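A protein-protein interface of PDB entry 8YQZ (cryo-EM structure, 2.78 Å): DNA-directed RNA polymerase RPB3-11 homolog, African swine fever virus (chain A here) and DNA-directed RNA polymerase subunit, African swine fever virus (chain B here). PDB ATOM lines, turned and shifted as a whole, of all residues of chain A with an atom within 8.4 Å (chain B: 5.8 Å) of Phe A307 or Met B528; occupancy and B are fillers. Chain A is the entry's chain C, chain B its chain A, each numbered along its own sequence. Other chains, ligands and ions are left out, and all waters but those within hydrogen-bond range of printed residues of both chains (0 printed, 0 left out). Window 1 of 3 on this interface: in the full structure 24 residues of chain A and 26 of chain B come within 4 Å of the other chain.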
ATOM      1  N   LYS A 276      16.951  23.557  -7.595  1.00  0.00           N
ATOM      2  CA  LYS A 276      15.819  22.981  -6.888  1.00  0.00           C
ATOM      3  C   LYS A 276      14.614  22.874  -7.814  1.00  0.00           C
ATOM      4  O   LYS A 276      14.320  23.788  -8.586  1.00  0.00           O
ATOM      5  CB  LYS A 276      15.474  23.827  -5.657  1.00  0.00           C
ATOM      6  CG  LYS A 276      14.973  23.033  -4.469  1.00  0.00           C
ATOM      7  CD  LYS A 276      14.696  23.926  -3.279  1.00  0.00           C
ATOM      8  CE  LYS A 276      15.952  24.436  -2.621  1.00  0.00           C
ATOM      9  NZ  LYS A 276      16.737  23.332  -2.038  1.00  0.00           N
ATOM     10  N   THR A 277      13.908  21.750  -7.721  1.00  0.00           N
ATOM     11  CA  THR A 277      12.766  21.455  -8.576  1.00  0.00           C
ATOM     12  C   THR A 277      11.545  21.189  -7.706  1.00  0.00           C
ATOM     13  O   THR A 277      11.658  20.587  -6.639  1.00  0.00           O
ATOM     14  CB  THR A 277      13.047  20.242  -9.470  1.00  0.00           C
ATOM     15  OG1 THR A 277      14.268  20.452 -10.182  1.00  0.00           O
ATOM     16  CG2 THR A 277      11.941  20.050 -10.478  1.00  0.00           C
ATOM     17  N   LYS A 278      10.382  21.639  -8.163  1.00  0.00           N
ATOM     18  CA  LYS A 278       9.141  21.521  -7.410  1.00  0.00           C
ATOM     19  C   LYS A 278       8.077  20.838  -8.254  1.00  0.00           C
ATOM     20  O   LYS A 278       7.851  21.225  -9.401  1.00  0.00           O
ATOM     21  CB  LYS A 278       8.670  22.900  -6.971  1.00  0.00           C
ATOM     22  CG  LYS A 278       7.428  22.918  -6.148  1.00  0.00           C
ATOM     23  CD  LYS A 278       7.092  24.333  -5.795  1.00  0.00           C
ATOM     24  CE  LYS A 278       5.910  24.402  -4.885  1.00  0.00           C
ATOM     25  NZ  LYS A 278       5.609  25.805  -4.549  1.00  0.00           N
ATOM     26  N   ALA A 279       7.418  19.834  -7.685  1.00  0.00           N
ATOM     27  CA  ALA A 279       6.374  19.079  -8.366  1.00  0.00           C
ATOM     28  C   ALA A 279       5.091  19.156  -7.558  1.00  0.00           C
ATOM     29  O   ALA A 279       5.120  19.022  -6.334  1.00  0.00           O
ATOM     30  CB  ALA A 279       6.786  17.622  -8.557  1.00  0.00           C
ATOM     31  N   LYS A 295       3.337   9.908   0.158  1.00  0.00           N
ATOM     32  CA  LYS A 295       4.274  10.684   0.960  1.00  0.00           C
ATOM     33  C   LYS A 295       5.247   9.783   1.707  1.00  0.00           C
ATOM     34  O   LYS A 295       6.454  10.041   1.723  1.00  0.00           O
ATOM     35  CB  LYS A 295       3.521  11.587   1.933  1.00  0.00           C
ATOM     36  CG  LYS A 295       4.442  12.343   2.862  1.00  0.00           C
ATOM     37  CD  LYS A 295       3.730  13.401   3.636  1.00  0.00           C
ATOM     38  CE  LYS A 295       2.826  12.819   4.679  1.00  0.00           C
ATOM     39  NZ  LYS A 295       3.569  12.027   5.666  1.00  0.00           N
ATOM     40  N   ILE A 298       7.771   8.162  -0.874  1.00  0.00           N
ATOM     41  CA  ILE A 298       8.688   9.175  -1.384  1.00  0.00           C
ATOM     42  C   ILE A 298       9.706   9.543  -0.316  1.00  0.00           C
ATOM     43  O   ILE A 298      10.894   9.715  -0.606  1.00  0.00           O
ATOM     44  CB  ILE A 298       7.907  10.409  -1.868  1.00  0.00           C
ATOM     45  CG1 ILE A 298       7.143  10.095  -3.143  1.00  0.00           C
ATOM     46  CG2 ILE A 298       8.842  11.555  -2.139  1.00  0.00           C
ATOM     47  CD1 ILE A 298       6.068  11.099  -3.472  1.00  0.00           C
ATOM     48  N   TYR A 299       9.262   9.668   0.934  1.00  0.00           N
ATOM     49  CA  TYR A 299      10.174  10.003   2.019  1.00  0.00           C
ATOM     50  C   TYR A 299      11.163   8.876   2.296  1.00  0.00           C
ATOM     51  O   TYR A 299      12.316   9.132   2.654  1.00  0.00           O
ATOM     52  CB  TYR A 299       9.364  10.349   3.262  1.00  0.00           C
ATOM     53  CG  TYR A 299      10.172  10.780   4.450  1.00  0.00           C
ATOM     54  CD1 TYR A 299      11.021  11.865   4.377  1.00  0.00           C
ATOM     55  CD2 TYR A 299      10.061  10.118   5.653  1.00  0.00           C
ATOM     56  CE1 TYR A 299      11.749  12.260   5.460  1.00  0.00           C
ATOM     57  CE2 TYR A 299      10.782  10.508   6.737  1.00  0.00           C
ATOM     58  CZ  TYR A 299      11.623  11.582   6.637  1.00  0.00           C
ATOM     59  OH  TYR A 299      12.343  11.973   7.727  1.00  0.00           O
ATOM     60  N   ILE A 302      13.785   9.155  -0.634  1.00  0.00           N
ATOM     61  CA  ILE A 302      14.639  10.335  -0.538  1.00  0.00           C
ATOM     62  C   ILE A 302      14.681  10.805   0.908  1.00  0.00           C
ATOM     63  O   ILE A 302      13.886  11.668   1.296  1.00  0.00           O
ATOM     64  CB  ILE A 302      14.138  11.467  -1.445  1.00  0.00           C
ATOM     65  CG1 ILE A 302      13.644  10.921  -2.779  1.00  0.00           C
ATOM     66  CG2 ILE A 302      15.231  12.461  -1.674  1.00  0.00           C
ATOM     67  CD1 ILE A 302      12.808  11.897  -3.559  1.00  0.00           C
ATOM     68  N   PRO A 303      15.577  10.273   1.738  1.00  0.00           N
ATOM     69  CA  PRO A 303      15.633  10.714   3.140  1.00  0.00           C
ATOM     70  C   PRO A 303      16.029  12.169   3.316  1.00  0.00           C
ATOM     71  O   PRO A 303      15.706  12.766   4.348  1.00  0.00           O
ATOM     72  CB  PRO A 303      16.676   9.773   3.752  1.00  0.00           C
ATOM     73  CG  PRO A 303      16.751   8.630   2.823  1.00  0.00           C
ATOM     74  CD  PRO A 303      16.515   9.178   1.475  1.00  0.00           C
ATOM     75  N   ASP A 304      16.732  12.755   2.351  1.00  0.00           N
ATOM     76  CA  ASP A 304      17.285  14.104   2.452  1.00  0.00           C
ATOM     77  C   ASP A 304      16.521  15.105   1.601  1.00  0.00           C
ATOM     78  O   ASP A 304      17.121  15.966   0.959  1.00  0.00           O
ATOM     79  CB  ASP A 304      18.758  14.098   2.068  1.00  0.00           C
ATOM     80  CG  ASP A 304      19.030  13.285   0.823  1.00  0.00           C
ATOM     81  OD1 ASP A 304      19.659  13.816  -0.117  1.00  0.00           O
ATOM     82  OD2 ASP A 304      18.626  12.106   0.781  1.00  0.00           O
ATOM     83  N   ILE A 305      15.194  15.002   1.573  1.00  0.00           N
ATOM     84  CA  ILE A 305      14.383  15.849   0.714  1.00  0.00           C
ATOM     85  C   ILE A 305      14.124  17.184   1.397  1.00  0.00           C
ATOM     86  O   ILE A 305      14.185  17.293   2.624  1.00  0.00           O
ATOM     87  CB  ILE A 305      13.079  15.116   0.356  1.00  0.00           C
ATOM     88  CG1 ILE A 305      12.403  15.757  -0.848  1.00  0.00           C
ATOM     89  CG2 ILE A 305      12.149  15.054   1.541  1.00  0.00           C
ATOM     90  CD1 ILE A 305      11.388  14.883  -1.484  1.00  0.00           C
ATOM     91  N   SER A 306      13.868  18.221   0.596  1.00  0.00           N
ATOM     92  CA  SER A 306      13.545  19.524   1.163  1.00  0.00           C
ATOM     93  C   SER A 306      12.147  19.539   1.754  1.00  0.00           C
ATOM     94  O   SER A 306      11.946  20.030   2.865  1.00  0.00           O
ATOM     95  CB  SER A 306      13.678  20.610   0.104  1.00  0.00           C
ATOM     96  OG  SER A 306      14.981  20.632  -0.426  1.00  0.00           O
ATOM     97  N   PHE A 307      11.172  18.999   1.034  1.00  0.00           N
ATOM     98  CA  PHE A 307       9.807  18.989   1.522  1.00  0.00           C
ATOM     99  C   PHE A 307       9.010  17.951   0.758  1.00  0.00           C
ATOM    100  O   PHE A 307       9.142  17.837  -0.457  1.00  0.00           O
ATOM    101  CB  PHE A 307       9.155  20.368   1.376  1.00  0.00           C
ATOM    102  CG  PHE A 307       7.787  20.446   1.960  1.00  0.00           C
ATOM    103  CD1 PHE A 307       7.613  20.526   3.323  1.00  0.00           C
ATOM    104  CD2 PHE A 307       6.674  20.429   1.150  1.00  0.00           C
ATOM    105  CE1 PHE A 307       6.362  20.585   3.863  1.00  0.00           C
ATOM    106  CE2 PHE A 307       5.423  20.491   1.690  1.00  0.00           C
ATOM    107  CZ  PHE A 307       5.268  20.569   3.051  1.00  0.00           C
ATOM    108  N   VAL A 308       8.195  17.190   1.479  1.00  0.00           N
ATOM    109  CA  VAL A 308       7.135  16.390   0.882  1.00  0.00           C
ATOM    110  C   VAL A 308       5.912  16.525   1.777  1.00  0.00           C
ATOM    111  O   VAL A 308       6.033  16.527   3.005  1.00  0.00           O
ATOM    112  CB  VAL A 308       7.546  14.914   0.678  1.00  0.00           C
ATOM    113  CG1 VAL A 308       7.829  14.215   1.989  1.00  0.00           C
ATOM    114  CG2 VAL A 308       6.504  14.174  -0.126  1.00  0.00           C
ATOM    115  N   GLY A 309       4.745  16.696   1.167  1.00  0.00           N
ATOM    116  CA  GLY A 309       3.519  16.829   1.928  1.00  0.00           C
ATOM    117  C   GLY A 309       2.322  16.743   1.016  1.00  0.00           C
ATOM    118  O   GLY A 309       2.422  16.953  -0.190  1.00  0.00           O
ATOM    119  N   TYR A 310       1.178  16.430   1.611  1.00  0.00           N
ATOM    120  CA  TYR A 310      -0.050  16.258   0.854  1.00  0.00           C
ATOM    121  C   TYR A 310      -1.184  16.951   1.586  1.00  0.00           C
ATOM    122  O   TYR A 310      -1.065  17.316   2.752  1.00  0.00           O
ATOM    123  CB  TYR A 310      -0.370  14.774   0.612  1.00  0.00           C
ATOM    124  CG  TYR A 310      -1.046  14.075   1.763  1.00  0.00           C
ATOM    125  CD1 TYR A 310      -0.308  13.575   2.813  1.00  0.00           C
ATOM    126  CD2 TYR A 310      -2.417  13.900   1.791  1.00  0.00           C
ATOM    127  CE1 TYR A 310      -0.906  12.949   3.853  1.00  0.00           C
ATOM    128  CE2 TYR A 310      -3.022  13.272   2.831  1.00  0.00           C
ATOM    129  CZ  TYR A 310      -2.262  12.795   3.864  1.00  0.00           C
ATOM    130  OH  TYR A 310      -2.850  12.150   4.926  1.00  0.00           O
ATOM    131  N   VAL A 320      -3.715  16.943  -3.212  1.00  0.00           N
ATOM    132  CA  VAL A 320      -2.605  17.699  -3.781  1.00  0.00           C
ATOM    133  C   VAL A 320      -1.325  17.266  -3.087  1.00  0.00           C
ATOM    134  O   VAL A 320      -1.191  17.431  -1.873  1.00  0.00           O
ATOM    135  CB  VAL A 320      -2.807  19.213  -3.628  1.00  0.00           C
ATOM    136  CG1 VAL A 320      -1.701  19.963  -4.332  1.00  0.00           C
ATOM    137  CG2 VAL A 320      -4.150  19.627  -4.155  1.00  0.00           C
ATOM    138  N   LEU A 321      -0.375  16.752  -3.854  1.00  0.00           N
ATOM    139  CA  LEU A 321       0.911  16.316  -3.331  1.00  0.00           C
ATOM    140  C   LEU A 321       2.001  17.264  -3.816  1.00  0.00           C
ATOM    141  O   LEU A 321       2.126  17.502  -5.016  1.00  0.00           O
ATOM    142  CB  LEU A 321       1.205  14.882  -3.762  1.00  0.00           C
ATOM    143  CG  LEU A 321       2.537  14.272  -3.332  1.00  0.00           C
ATOM    144  CD1 LEU A 321       2.516  13.834  -1.890  1.00  0.00           C
ATOM    145  CD2 LEU A 321       2.887  13.122  -4.232  1.00  0.00           C
ATOM    146  N   THR A 322       2.793  17.787  -2.889  1.00  0.00           N
ATOM    147  CA  THR A 322       3.857  18.734  -3.192  1.00  0.00           C
ATOM    148  C   THR A 322       5.206  18.119  -2.855  1.00  0.00           C
ATOM    149  O   THR A 322       5.398  17.608  -1.751  1.00  0.00           O
ATOM    150  CB  THR A 322       3.678  20.035  -2.408  1.00  0.00           C
ATOM    151  OG1 THR A 322       2.378  20.575  -2.653  1.00  0.00           O
ATOM    152  CG2 THR A 322       4.717  21.049  -2.817  1.00  0.00           C
ATOM    153  N   ILE A 323       6.139  18.178  -3.802  1.00  0.00           N
ATOM    154  CA  ILE A 323       7.497  17.686  -3.612  1.00  0.00           C
ATOM    155  C   ILE A 323       8.463  18.794  -3.994  1.00  0.00           C
ATOM    156  O   ILE A 323       8.299  19.432  -5.035  1.00  0.00           O
ATOM    157  CB  ILE A 323       7.772  16.420  -4.443  1.00  0.00           C
ATOM    158  CG1 ILE A 323       6.742  15.348  -4.119  1.00  0.00           C
ATOM    159  CG2 ILE A 323       9.153  15.896  -4.175  1.00  0.00           C
ATOM    160  CD1 ILE A 323       6.458  14.441  -5.249  1.00  0.00           C
ATOM    161  N   ILE A 324       9.450  19.043  -3.144  1.00  0.00           N
ATOM    162  CA  ILE A 324      10.510  20.003  -3.423  1.00  0.00           C
ATOM    163  C   ILE A 324      11.831  19.296  -3.189  1.00  0.00           C
ATOM    164  O   ILE A 324      12.106  18.849  -2.074  1.00  0.00           O
ATOM    165  CB  ILE A 324      10.397  21.260  -2.547  1.00  0.00           C
ATOM    166  CG1 ILE A 324       9.127  22.025  -2.896  1.00  0.00           C
ATOM    167  CG2 ILE A 324      11.583  22.140  -2.744  1.00  0.00           C
ATOM    168  CD1 ILE A 324       8.770  23.079  -1.932  1.00  0.00           C
ATOM    169  N   HIS A 325      12.644  19.185  -4.233  1.00  0.00           N
ATOM    170  CA  HIS A 325      13.883  18.436  -4.135  1.00  0.00           C
ATOM    171  C   HIS A 325      14.972  19.160  -4.907  1.00  0.00           C
ATOM    172  O   HIS A 325      14.705  19.945  -5.815  1.00  0.00           O
ATOM    173  CB  HIS A 325      13.717  17.003  -4.649  1.00  0.00           C
ATOM    174  CG  HIS A 325      14.885  16.117  -4.357  1.00  0.00           C
ATOM    175  ND1 HIS A 325      15.538  16.122  -3.146  1.00  0.00           N
ATOM    176  CD2 HIS A 325      15.506  15.185  -5.114  1.00  0.00           C
ATOM    177  CE1 HIS A 325      16.518  15.239  -3.173  1.00  0.00           C
ATOM    178  NE2 HIS A 325      16.520  14.655  -4.355  1.00  0.00           N
ATOM    179  N   LYS A 326      16.213  18.853  -4.545  1.00  0.00           N
ATOM    180  CA  LYS A 326      17.408  19.521  -5.055  1.00  0.00           C
ATOM    181  C   LYS A 326      17.980  18.815  -6.273  1.00  0.00           C
ATOM    182  O   LYS A 326      19.195  18.741  -6.432  1.00  0.00           O
ATOM    183  CB  LYS A 326      18.456  19.607  -3.957  1.00  0.00           C
ATOM    184  CG  LYS A 326      18.690  20.992  -3.409  1.00  0.00           C
ATOM    185  CD  LYS A 326      19.697  20.950  -2.265  1.00  0.00           C
ATOM    186  CE  LYS A 326      19.134  21.580  -1.000  1.00  0.00           C
ATOM    187  NZ  LYS A 326      20.148  21.760   0.077  1.00  0.00           N
ATOM    188  N   LEU A 332      14.171  13.765 -10.573  1.00  0.00           N
ATOM    189  CA  LEU A 332      13.034  13.720  -9.665  1.00  0.00           C
ATOM    190  C   LEU A 332      11.981  12.734 -10.146  1.00  0.00           C
ATOM    191  O   LEU A 332      11.455  11.944  -9.356  1.00  0.00           O
ATOM    192  CB  LEU A 332      12.434  15.113  -9.509  1.00  0.00           C
ATOM    193  CG  LEU A 332      11.296  15.215  -8.496  1.00  0.00           C
ATOM    194  CD1 LEU A 332      11.791  14.756  -7.149  1.00  0.00           C
ATOM    195  CD2 LEU A 332      10.770  16.625  -8.420  1.00  0.00           C
ATOM    196  N   ASN B 523      10.234  14.360  14.954  1.00  0.00           N
ATOM    197  CA  ASN B 523      11.212  14.013  13.937  1.00  0.00           C
ATOM    198  C   ASN B 523      10.942  14.795  12.651  1.00  0.00           C
ATOM    199  O   ASN B 523      10.013  15.594  12.562  1.00  0.00           O
ATOM    200  CB  ASN B 523      11.237  12.501  13.705  1.00  0.00           C
ATOM    201  CG  ASN B 523       9.905  11.935  13.268  1.00  0.00           C
ATOM    202  OD1 ASN B 523       8.971  12.658  12.981  1.00  0.00           O
ATOM    203  ND2 ASN B 523       9.815  10.623  13.237  1.00  0.00           N
ATOM    204  N   LYS B 524      11.774  14.570  11.637  1.00  0.00           N
ATOM    205  CA  LYS B 524      11.702  15.377  10.426  1.00  0.00           C
ATOM    206  C   LYS B 524      10.379  15.189   9.696  1.00  0.00           C
ATOM    207  O   LYS B 524       9.856  16.132   9.098  1.00  0.00           O
ATOM    208  CB  LYS B 524      12.872  15.043   9.505  1.00  0.00           C
ATOM    209  CG  LYS B 524      12.838  15.762   8.189  1.00  0.00           C
ATOM    210  CD  LYS B 524      13.912  15.277   7.268  1.00  0.00           C
ATOM    211  CE  LYS B 524      13.787  15.897   5.904  1.00  0.00           C
ATOM    212  NZ  LYS B 524      14.948  15.555   5.071  1.00  0.00           N
ATOM    213  N   LEU B 525       9.834  13.976   9.710  1.00  0.00           N
ATOM    214  CA  LEU B 525       8.587  13.717   9.006  1.00  0.00           C
ATOM    215  C   LEU B 525       7.425  14.485   9.617  1.00  0.00           C
ATOM    216  O   LEU B 525       6.575  15.017   8.896  1.00  0.00           O
ATOM    217  CB  LEU B 525       8.298  12.223   9.012  1.00  0.00           C
ATOM    218  CG  LEU B 525       7.014  11.764   8.334  1.00  0.00           C
ATOM    219  CD1 LEU B 525       7.063  12.019   6.854  1.00  0.00           C
ATOM    220  CD2 LEU B 525       6.815  10.311   8.612  1.00  0.00           C
ATOM    221  N   HIS B 526       7.359  14.537  10.944  1.00  0.00           N
ATOM    222  CA  HIS B 526       6.275  15.231  11.620  1.00  0.00           C
ATOM    223  C   HIS B 526       6.456  16.735  11.630  1.00  0.00           C
ATOM    224  O   HIS B 526       5.464  17.465  11.655  1.00  0.00           O
ATOM    225  CB  HIS B 526       6.129  14.708  13.040  1.00  0.00           C
ATOM    226  CG  HIS B 526       5.534  13.342  13.103  1.00  0.00           C
ATOM    227  ND1 HIS B 526       6.279  12.199  12.928  1.00  0.00           N
ATOM    228  CD2 HIS B 526       4.256  12.938  13.255  1.00  0.00           C
ATOM    229  CE1 HIS B 526       5.490  11.147  13.008  1.00  0.00           C
ATOM    230  NE2 HIS B 526       4.256  11.568  13.203  1.00  0.00           N
ATOM    231  N   ALA B 527       7.698  17.217  11.638  1.00  0.00           N
ATOM    232  CA  ALA B 527       7.938  18.645  11.487  1.00  0.00           C
ATOM    233  C   ALA B 527       7.550  19.124  10.097  1.00  0.00           C
ATOM    234  O   ALA B 527       6.994  20.214   9.945  1.00  0.00           O
ATOM    235  CB  ALA B 527       9.399  18.963  11.777  1.00  0.00           C
ATOM    236  N   MET B 528       7.837  18.326   9.074  1.00  0.00           N
ATOM    237  CA  MET B 528       7.399  18.649   7.722  1.00  0.00           C
ATOM    238  C   MET B 528       5.881  18.634   7.616  1.00  0.00           C
ATOM    239  O   MET B 528       5.299  19.408   6.852  1.00  0.00           O
ATOM    240  CB  MET B 528       8.017  17.662   6.736  1.00  0.00           C
ATOM    241  CG  MET B 528       9.232  18.165   6.025  1.00  0.00           C
ATOM    242  SD  MET B 528       9.803  17.141   4.673  1.00  0.00           S
ATOM    243  CE  MET B 528       9.354  15.525   5.260  1.00  0.00           C
ATOM    244  N   GLY B 529       5.223  17.753   8.368  1.00  0.00           N
ATOM    245  CA  GLY B 529       3.783  17.622   8.302  1.00  0.00           C
ATOM    246  C   GLY B 529       3.017  18.777   8.900  1.00  0.00           C
ATOM    247  O   GLY B 529       1.865  18.990   8.532  1.00  0.00           O
ATOM    248  N   LEU B 530       3.623  19.522   9.819  1.00  0.00           N
ATOM    249  CA  LEU B 530       2.974  20.701  10.375  1.00  0.00           C
ATOM    250  C   LEU B 530       2.764  21.792   9.341  1.00  0.00           C
ATOM    251  O   LEU B 530       1.873  22.623   9.511  1.00  0.00           O
ATOM    252  CB  LEU B 530       3.793  21.251  11.539  1.00  0.00           C
ATOM    253  CG  LEU B 530       3.395  20.922  12.975  1.00  0.00           C
ATOM    254  CD1 LEU B 530       2.989  19.495  13.157  1.00  0.00           C
ATOM    255  CD2 LEU B 530       4.524  21.267  13.880  1.00  0.00           C
ATOM    256  N   PHE B 531       3.553  21.800   8.276  1.00  0.00           N
ATOM    257  CA  PHE B 531       3.496  22.831   7.259  1.00  0.00           C
ATOM    258  C   PHE B 531       2.729  22.419   6.013  1.00  0.00           C
ATOM    259  O   PHE B 531       2.634  23.217   5.082  1.00  0.00           O
ATOM    260  CB  PHE B 531       4.911  23.233   6.845  1.00  0.00           C
ATOM    261  CG  PHE B 531       5.622  24.074   7.843  1.00  0.00           C
ATOM    262  CD1 PHE B 531       5.461  25.440   7.855  1.00  0.00           C
ATOM    263  CD2 PHE B 531       6.465  23.498   8.765  1.00  0.00           C
ATOM    264  CE1 PHE B 531       6.124  26.201   8.765  1.00  0.00           C
ATOM    265  CE2 PHE B 531       7.120  24.256   9.667  1.00  0.00           C
ATOM    266  CZ  PHE B 531       6.947  25.608   9.671  1.00  0.00           C
ATOM    267  N   GLN B 532       2.192  21.212   5.955  1.00  0.00           N
ATOM    268  CA  GLN B 532       1.588  20.772   4.708  1.00  0.00           C
ATOM    269  C   GLN B 532       0.185  21.304   4.522  1.00  0.00           C
ATOM    270  O   GLN B 532      -0.525  20.850   3.627  1.00  0.00           O
ATOM    271  CB  GLN B 532       1.608  19.248   4.597  1.00  0.00           C
ATOM    272  CG  GLN B 532       0.781  18.499   5.573  1.00  0.00           C
ATOM    273  CD  GLN B 532       1.034  17.015   5.487  1.00  0.00           C
ATOM    274  OE1 GLN B 532       1.831  16.568   4.684  1.00  0.00           O
ATOM    275  NE2 GLN B 532       0.382  16.251   6.335  1.00  0.00           N
ATOM    276  N   PRO B 538       6.717  26.245   1.568  1.00  0.00           N
ATOM    277  CA  PRO B 538       7.287  25.341   2.561  1.00  0.00           C
ATOM    278  C   PRO B 538       8.704  25.741   2.924  1.00  0.00           C
ATOM    279  O   PRO B 538       9.440  26.289   2.093  1.00  0.00           O
ATOM    280  CB  PRO B 538       7.260  23.983   1.853  1.00  0.00           C
ATOM    281  CG  PRO B 538       6.317  24.135   0.751  1.00  0.00           C
ATOM    282  CD  PRO B 538       6.406  25.546   0.317  1.00  0.00           C
ATOM    283  N   PRO B 539       9.121  25.496   4.153  1.00  0.00           N
ATOM    284  CA  PRO B 539      10.533  25.681   4.506  1.00  0.00           C
ATOM    285  C   PRO B 539      11.410  24.588   3.925  1.00  0.00           C
ATOM    286  O   PRO B 539      10.911  23.668   3.274  1.00  0.00           O
ATOM    287  CB  PRO B 539      10.518  25.634   6.038  1.00  0.00           C
ATOM    288  CG  PRO B 539       9.096  25.844   6.422  1.00  0.00           C
ATOM    289  CD  PRO B 539       8.294  25.241   5.338  1.00  0.00           C
ATOM    290  N   PHE B 541      13.995  21.499   4.649  1.00  0.00           N
ATOM    291  CA  PHE B 541      14.438  20.542   5.650  1.00  0.00           C
ATOM    292  C   PHE B 541      15.593  19.694   5.142  1.00  0.00           C
ATOM    293  O   PHE B 541      15.858  18.627   5.689  1.00  0.00           O
ATOM    294  CB  PHE B 541      13.281  19.638   6.082  1.00  0.00           C
ATOM    295  CG  PHE B 541      12.181  20.349   6.816  1.00  0.00           C
ATOM    296  CD1 PHE B 541      11.188  21.012   6.126  1.00  0.00           C
ATOM    297  CD2 PHE B 541      12.118  20.330   8.189  1.00  0.00           C
ATOM    298  CE1 PHE B 541      10.175  21.648   6.791  1.00  0.00           C
ATOM    299  CE2 PHE B 541      11.103  20.976   8.849  1.00  0.00           C
ATOM    300  CZ  PHE B 541      10.137  21.632   8.149  1.00  0.00           C
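NZ of Lys B524 is in hydrogen-bond range of O of Pro A303 (3.0 Å). The side-chain amino group of Lys B524 sits at hydrogen-bond distance from the backbone carbonyl oxygen of Ile A305, at 3.1 Å. The side-chain sulfur (SD) of Met B528 is in hydrogen-bond range of the backbone NH (N) of Val A308 (3.6 Å). OE1 of Gln B532 sits at hydrogen-bond distance from N of Tyr A310. N of Phe B541 lies within hydrogen-bond range of O of Ser A306 (3.1 Å).
The side-chain amino group (NZ) of Lys B524 is in hydrogen-bond range of the backbone carbonyl oxygen (O) of Phe B541, 3.3 Å away. The backbone NH (N) of Ser A306 lies close to the backbone carbonyl oxygen (O) of Ile A324 (3.3 Å). The backbone carbonyl oxygen (O) of Phe A307 sits at hydrogen-bond distance from the backbone NH (N) of Ile A324 (3.0 Å). O of Gly A309 is in hydrogen-bond range of N of Thr A322, 2.8 Å away.
Lys A295 touches Leu B525 (NZ to CD1, 3.7 Å). OE1 of Gln B532 touches CD of Lys A295 (3.8 Å). Lys B524 touches Tyr A299. Tyr A299 touches Leu B525. Asp A304 touches Lys B524. Ser A306 touches Pro B539. CE1 of Phe A307 touches O of Met B528 (3.4 Å). Pro B538 touches Phe A307. Gln B532 touches Gly A309. Pro B538 touches Ile A324.
Printed residues of chain B within 4 Å of Asp A304: Lys B524 (3.8 Å). Of the printed residues of chain B, Phe A307 touches Met B528 and Pro B538. Of the printed residues of chain B, Tyr A310 touches Gln B532. No residue of chain A comes within 4 Å of Ala B527. Of chain A, only Phe A307 and Val A308 come within 4 Å of Met B528. The nearest printed residue of chain B that does not touch Asp A304 is Phe B541 (5.4 Å).
Along chain B the printed residues that touch a printed residue of chain A span positions 524 to 541. Among the printed residues, no Asp or Glu carboxylate lies within 4 Å of a Lys or Arg side-chain nitrogen of the other chain.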
